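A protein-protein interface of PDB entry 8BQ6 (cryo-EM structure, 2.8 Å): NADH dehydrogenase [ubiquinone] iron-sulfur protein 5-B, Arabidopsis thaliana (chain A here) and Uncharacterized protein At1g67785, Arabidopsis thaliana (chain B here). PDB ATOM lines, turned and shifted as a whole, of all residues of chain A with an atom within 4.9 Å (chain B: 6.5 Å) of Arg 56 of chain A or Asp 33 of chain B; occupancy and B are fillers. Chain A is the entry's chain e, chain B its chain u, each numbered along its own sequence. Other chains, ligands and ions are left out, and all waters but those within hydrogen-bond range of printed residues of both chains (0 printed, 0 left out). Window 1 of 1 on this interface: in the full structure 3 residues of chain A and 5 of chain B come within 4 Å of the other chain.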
ATOM      1  N   GLN A  52       9.051  16.466  19.943  1.00  0.00           N
ATOM      2  CA  GLN A  52       8.261  17.492  20.613  1.00  0.00           C
ATOM      3  C   GLN A  52       7.068  16.882  21.341  1.00  0.00           C
ATOM      4  O   GLN A  52       6.784  17.234  22.491  1.00  0.00           O
ATOM      5  CB  GLN A  52       7.800  18.528  19.595  1.00  0.00           C
ATOM      6  CG  GLN A  52       8.187  19.940  19.945  1.00  0.00           C
ATOM      7  CD  GLN A  52       7.776  20.920  18.874  1.00  0.00           C
ATOM      8  OE1 GLN A  52       7.897  20.638  17.682  1.00  0.00           O
ATOM      9  NE2 GLN A  52       7.289  22.083  19.289  1.00  0.00           N
ATOM     10  N   ARG A  53       6.364  15.955  20.687  1.00  0.00           N
ATOM     11  CA  ARG A  53       5.225  15.303  21.326  1.00  0.00           C
ATOM     12  C   ARG A  53       5.654  14.472  22.536  1.00  0.00           C
ATOM     13  O   ARG A  53       4.997  14.499  23.593  1.00  0.00           O
ATOM     14  CB  ARG A  53       4.503  14.437  20.301  1.00  0.00           C
ATOM     15  CG  ARG A  53       3.672  13.338  20.901  1.00  0.00           C
ATOM     16  CD  ARG A  53       3.548  12.176  19.937  1.00  0.00           C
ATOM     17  NE  ARG A  53       2.378  11.350  20.211  1.00  0.00           N
ATOM     18  CZ  ARG A  53       1.124  11.778  20.144  1.00  0.00           C
ATOM     19  NH1 ARG A  53       0.833  13.030  19.823  1.00  0.00           N
ATOM     20  NH2 ARG A  53       0.135  10.927  20.392  1.00  0.00           N
ATOM     21  N   ARG A  54       6.750  13.722  22.407  1.00  0.00           N
ATOM     22  CA  ARG A  54       7.222  12.945  23.549  1.00  0.00           C
ATOM     23  C   ARG A  54       7.682  13.843  24.690  1.00  0.00           C
ATOM     24  O   ARG A  54       7.532  13.488  25.867  1.00  0.00           O
ATOM     25  CB  ARG A  54       8.338  11.999  23.124  1.00  0.00           C
ATOM     26  CG  ARG A  54       7.812  10.739  22.486  1.00  0.00           C
ATOM     27  CD  ARG A  54       8.808  10.154  21.525  1.00  0.00           C
ATOM     28  NE  ARG A  54       9.698   9.203  22.175  1.00  0.00           N
ATOM     29  CZ  ARG A  54      10.573   8.450  21.526  1.00  0.00           C
ATOM     30  NH1 ARG A  54      10.697   8.517  20.212  1.00  0.00           N
ATOM     31  NH2 ARG A  54      11.340   7.608  22.211  1.00  0.00           N
ATOM     32  N   ASN A  55       8.227  15.014  24.367  1.00  0.00           N
ATOM     33  CA  ASN A  55       8.591  15.954  25.416  1.00  0.00           C
ATOM     34  C   ASN A  55       7.356  16.529  26.089  1.00  0.00           C
ATOM     35  O   ASN A  55       7.385  16.794  27.292  1.00  0.00           O
ATOM     36  CB  ASN A  55       9.466  17.066  24.849  1.00  0.00           C
ATOM     37  CG  ASN A  55      10.848  16.575  24.473  1.00  0.00           C
ATOM     38  OD1 ASN A  55      11.251  15.474  24.844  1.00  0.00           O
ATOM     39  ND2 ASN A  55      11.592  17.403  23.756  1.00  0.00           N
ATOM     40  N   ARG A  56       6.275  16.735  25.332  1.00  0.00           N
ATOM     41  CA  ARG A  56       5.004  17.117  25.943  1.00  0.00           C
ATOM     42  C   ARG A  56       4.554  16.078  26.957  1.00  0.00           C
ATOM     43  O   ARG A  56       4.115  16.422  28.064  1.00  0.00           O
ATOM     44  CB  ARG A  56       3.928  17.280  24.874  1.00  0.00           C
ATOM     45  CG  ARG A  56       4.173  18.370  23.871  1.00  0.00           C
ATOM     46  CD  ARG A  56       2.866  19.026  23.480  1.00  0.00           C
ATOM     47  NE  ARG A  56       3.079  20.197  22.641  1.00  0.00           N
ATOM     48  CZ  ARG A  56       3.321  20.151  21.338  1.00  0.00           C
ATOM     49  NH1 ARG A  56       3.360  19.003  20.682  1.00  0.00           N
ATOM     50  NH2 ARG A  56       3.531  21.286  20.677  1.00  0.00           N
ATOM     51  N   ILE A  57       4.642  14.800  26.588  1.00  0.00           N
ATOM     52  CA  ILE A  57       4.254  13.737  27.516  1.00  0.00           C
ATOM     53  C   ILE A  57       5.117  13.787  28.771  1.00  0.00           C
ATOM     54  O   ILE A  57       4.618  13.703  29.901  1.00  0.00           O
ATOM     55  CB  ILE A  57       4.343  12.364  26.831  1.00  0.00           C
ATOM     56  CG1 ILE A  57       3.160  12.173  25.885  1.00  0.00           C
ATOM     57  CG2 ILE A  57       4.392  11.250  27.868  1.00  0.00           C
ATOM     58  CD1 ILE A  57       3.466  11.272  24.727  1.00  0.00           C
ATOM     59  N   TYR A  58       6.430  13.934  28.586  1.00  0.00           N
ATOM     60  CA  TYR A  58       7.335  13.981  29.729  1.00  0.00           C
ATOM     61  C   TYR A  58       7.048  15.189  30.620  1.00  0.00           C
ATOM     62  O   TYR A  58       7.082  15.088  31.852  1.00  0.00           O
ATOM     63  CB  TYR A  58       8.776  13.995  29.226  1.00  0.00           C
ATOM     64  CG  TYR A  58       9.764  14.612  30.175  1.00  0.00           C
ATOM     65  CD1 TYR A  58      10.302  13.879  31.222  1.00  0.00           C
ATOM     66  CD2 TYR A  58      10.155  15.934  30.028  1.00  0.00           C
ATOM     67  CE1 TYR A  58      11.209  14.446  32.090  1.00  0.00           C
ATOM     68  CE2 TYR A  58      11.053  16.509  30.892  1.00  0.00           C
ATOM     69  CZ  TYR A  58      11.578  15.763  31.919  1.00  0.00           C
ATOM     70  OH  TYR A  58      12.479  16.346  32.774  1.00  0.00           O
ATOM     71  N   LYS A  59       6.766  16.340  30.007  1.00  0.00           N
ATOM     72  CA  LYS A  59       6.447  17.551  30.754  1.00  0.00           C
ATOM     73  C   LYS A  59       5.179  17.372  31.574  1.00  0.00           C
ATOM     74  O   LYS A  59       5.106  17.799  32.730  1.00  0.00           O
ATOM     75  CB  LYS A  59       6.288  18.719  29.782  1.00  0.00           C
ATOM     76  CG  LYS A  59       6.681  20.075  30.320  1.00  0.00           C
ATOM     77  CD  LYS A  59       7.178  20.953  29.188  1.00  0.00           C
ATOM     78  CE  LYS A  59       6.986  22.429  29.494  1.00  0.00           C
ATOM     79  NZ  LYS A  59       6.252  23.113  28.395  1.00  0.00           N
ATOM     80  N   GLU A  60       4.155  16.755  30.980  1.00  0.00           N
ATOM     81  CA  GLU A  60       2.921  16.502  31.716  1.00  0.00           C
ATOM     82  C   GLU A  60       3.155  15.542  32.873  1.00  0.00           C
ATOM     83  O   GLU A  60       2.568  15.702  33.951  1.00  0.00           O
ATOM     84  CB  GLU A  60       1.851  15.955  30.781  1.00  0.00           C
ATOM     85  CG  GLU A  60       0.972  17.024  30.191  1.00  0.00           C
ATOM     86  CD  GLU A  60       0.024  17.594  31.220  1.00  0.00           C
ATOM     87  OE1 GLU A  60      -0.624  16.796  31.927  1.00  0.00           O
ATOM     88  OE2 GLU A  60      -0.080  18.836  31.315  1.00  0.00           O
ATOM     89  N   ALA B  29      14.912  22.762  25.065  1.00  0.00           N
ATOM     90  CA  ALA B  29      13.955  21.727  24.687  1.00  0.00           C
ATOM     91  C   ALA B  29      12.649  21.863  25.461  1.00  0.00           C
ATOM     92  O   ALA B  29      11.575  21.536  24.941  1.00  0.00           O
ATOM     93  CB  ALA B  29      14.561  20.343  24.909  1.00  0.00           C
ATOM     94  N   LEU B  30      12.719  22.336  26.706  1.00  0.00           N
ATOM     95  CA  LEU B  30      11.518  22.432  27.526  1.00  0.00           C
ATOM     96  C   LEU B  30      10.607  23.576  27.107  1.00  0.00           C
ATOM     97  O   LEU B  30       9.427  23.573  27.471  1.00  0.00           O
ATOM     98  CB  LEU B  30      11.891  22.584  28.999  1.00  0.00           C
ATOM     99  CG  LEU B  30      12.086  21.252  29.723  1.00  0.00           C
ATOM    100  CD1 LEU B  30      12.945  21.407  30.970  1.00  0.00           C
ATOM    101  CD2 LEU B  30      10.738  20.644  30.061  1.00  0.00           C
ATOM    102  N   HIS B  31      11.116  24.550  26.354  1.00  0.00           N
ATOM    103  CA  HIS B  31      10.332  25.715  25.968  1.00  0.00           C
ATOM    104  C   HIS B  31       9.989  25.730  24.487  1.00  0.00           C
ATOM    105  O   HIS B  31       9.908  26.808  23.889  1.00  0.00           O
ATOM    106  CB  HIS B  31      11.066  27.000  26.346  1.00  0.00           C
ATOM    107  CG  HIS B  31      11.337  27.128  27.810  1.00  0.00           C
ATOM    108  ND1 HIS B  31      10.337  27.328  28.736  1.00  0.00           N
ATOM    109  CD2 HIS B  31      12.495  27.097  28.508  1.00  0.00           C
ATOM    110  CE1 HIS B  31      10.866  27.404  29.943  1.00  0.00           C
ATOM    111  NE2 HIS B  31      12.175  27.275  29.832  1.00  0.00           N
ATOM    112  N   GLN B  32       9.787  24.563  23.878  1.00  0.00           N
ATOM    113  CA  GLN B  32       9.349  24.542  22.488  1.00  0.00           C
ATOM    114  C   GLN B  32       7.878  24.924  22.375  1.00  0.00           C
ATOM    115  O   GLN B  32       7.449  25.496  21.365  1.00  0.00           O
ATOM    116  CB  GLN B  32       9.605  23.165  21.879  1.00  0.00           C
ATOM    117  CG  GLN B  32      11.036  22.969  21.410  1.00  0.00           C
ATOM    118  CD  GLN B  32      11.518  24.108  20.529  1.00  0.00           C
ATOM    119  OE1 GLN B  32      12.321  24.939  20.951  1.00  0.00           O
ATOM    120  NE2 GLN B  32      11.030  24.148  19.296  1.00  0.00           N
ATOM    121  N   ASP B  33       7.095  24.640  23.418  1.00  0.00           N
ATOM    122  CA  ASP B  33       5.656  24.865  23.350  1.00  0.00           C
ATOM    123  C   ASP B  33       5.311  26.345  23.444  1.00  0.00           C
ATOM    124  O   ASP B  33       4.409  26.817  22.745  1.00  0.00           O
ATOM    125  CB  ASP B  33       4.954  24.075  24.449  1.00  0.00           C
ATOM    126  CG  ASP B  33       5.051  22.587  24.229  1.00  0.00           C
ATOM    127  OD1 ASP B  33       4.012  21.972  23.916  1.00  0.00           O
ATOM    128  OD2 ASP B  33       6.165  22.037  24.356  1.00  0.00           O
ATOM    129  N   GLU B  34       6.000  27.091  24.309  1.00  0.00           N
ATOM    130  CA  GLU B  34       5.777  28.531  24.352  1.00  0.00           C
ATOM    131  C   GLU B  34       6.206  29.189  23.049  1.00  0.00           C
ATOM    132  O   GLU B  34       5.547  30.118  22.572  1.00  0.00           O
ATOM    133  CB  GLU B  34       6.514  29.146  25.540  1.00  0.00           C
ATOM    134  CG  GLU B  34       5.856  28.846  26.870  1.00  0.00           C
ATOM    135  CD  GLU B  34       6.355  27.553  27.478  1.00  0.00           C
ATOM    136  OE1 GLU B  34       6.324  26.520  26.777  1.00  0.00           O
ATOM    137  OE2 GLU B  34       6.776  27.565  28.652  1.00  0.00           O
ATOM    138  N   LYS B  35       7.309  28.724  22.458  1.00  0.00           N
ATOM    139  CA  LYS B  35       7.690  29.230  21.144  1.00  0.00           C
ATOM    140  C   LYS B  35       6.589  28.973  20.128  1.00  0.00           C
ATOM    141  O   LYS B  35       6.228  29.865  19.349  1.00  0.00           O
ATOM    142  CB  LYS B  35       8.990  28.577  20.682  1.00  0.00           C
ATOM    143  CG  LYS B  35      10.245  29.276  21.143  1.00  0.00           C
ATOM    144  CD  LYS B  35      11.475  28.495  20.709  1.00  0.00           C
ATOM    145  CE  LYS B  35      11.382  28.073  19.249  1.00  0.00           C
ATOM    146  NZ  LYS B  35      11.571  29.218  18.317  1.00  0.00           N
ATOM    147  N   GLN B  36       6.031  27.763  20.139  1.00  0.00           N
ATOM    148  CA  GLN B  36       4.984  27.424  19.185  1.00  0.00           C
ATOM    149  C   GLN B  36       3.736  28.272  19.409  1.00  0.00           C
ATOM    150  O   GLN B  36       3.125  28.751  18.449  1.00  0.00           O
ATOM    151  CB  GLN B  36       4.677  25.930  19.285  1.00  0.00           C
ATOM    152  CG  GLN B  36       3.623  25.419  18.327  1.00  0.00           C
ATOM    153  CD  GLN B  36       2.398  24.886  19.038  1.00  0.00           C
ATOM    154  OE1 GLN B  36       2.338  24.861  20.268  1.00  0.00           O
ATOM    155  NE2 GLN B  36       1.416  24.440  18.264  1.00  0.00           N
ATOM    156  N   GLU B  37       3.358  28.492  20.672  1.00  0.00           N
ATOM    157  CA  GLU B  37       2.154  29.266  20.961  1.00  0.00           C
ATOM    158  C   GLU B  37       2.339  30.740  20.610  1.00  0.00           C
ATOM    159  O   GLU B  37       1.417  31.379  20.091  1.00  0.00           O
ATOM    160  CB  GLU B  37       1.743  29.085  22.428  1.00  0.00           C
ATOM    161  CG  GLU B  37       1.271  27.690  22.817  1.00  0.00           C
ATOM    162  CD  GLU B  37       0.948  27.557  24.295  1.00  0.00           C
ATOM    163  OE1 GLU B  37       1.268  28.488  25.063  1.00  0.00           O
ATOM    164  OE2 GLU B  37       0.379  26.515  24.685  1.00  0.00           O
ATOM    165  N   ARG B  38       3.525  31.298  20.873  1.00  0.00           N
ATOM    166  CA  ARG B  38       3.796  32.676  20.481  1.00  0.00           C
ATOM    167  C   ARG B  38       3.784  32.822  18.967  1.00  0.00           C
ATOM    168  O   ARG B  38       3.243  33.799  18.431  1.00  0.00           O
ATOM    169  CB  ARG B  38       5.139  33.132  21.046  1.00  0.00           C
ATOM    170  CG  ARG B  38       5.258  34.632  21.236  1.00  0.00           C
ATOM    171  CD  ARG B  38       4.551  35.072  22.501  1.00  0.00           C
ATOM    172  NE  ARG B  38       5.023  36.367  22.974  1.00  0.00           N
ATOM    173  CZ  ARG B  38       4.404  37.517  22.747  1.00  0.00           C
ATOM    174  NH1 ARG B  38       3.293  37.574  22.032  1.00  0.00           N
ATOM    175  NH2 ARG B  38       4.911  38.638  23.253  1.00  0.00           N
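NH2 of Arg 56 of chain A lies within salt-bridge range of OD1 of Asp 33 of chain B (3.3 Å).
The backbone carbonyl oxygen of Leu 30 of chain B lies within hydrogen-bond range of the side-chain amino group of Lys 59 of chain A (3.3 Å).
OE1 of Glu 34 of chain B lies within salt-bridge range of NZ of Lys 59 of chain A (3.8 Å).
Among the printed residues, merely in contact across the chains: Gln 52 of chain A with Gln 32 of chain B (3.6 Å) and Arg 56 of chain A with Gln 36 of chain B (3.8 Å).
Arg 56 of chain A touches two residues of chain B.
Asp 33 of chain B touches one residue of chain A.
Printed residues of chain B within 4 Å of Gln 52 of chain A: Gln 32 (3.6 Å).
Printed residues of chain A within 4 Å of Gln 36 of chain B: Arg 56.
Printed residues of chain A within 4 Å of Glu 34 of chain B: Lys 59 (3.8 Å).
Of the printed residues of chain A, Leu 30 of chain B touches Lys 59.
Of the printed residues of chain B, Lys 59 of chain A touches Leu 30 (3.3 Å) and Glu 34 (3.8 Å).
Asn 55 of chain A touches none of the printed residues of chain B.
The nearest residue of chain A that does not touch Asp 33 of chain B is Lys 59 of chain A (4.2 Å).
Among the printed residues, Asp or Glu carboxylates within 4 Å of a Lys or Arg side-chain nitrogen of the other chain: Arg 56 of chain A with Asp 33 of chain B and Lys 59 of chain A with Glu 34 of chain B.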
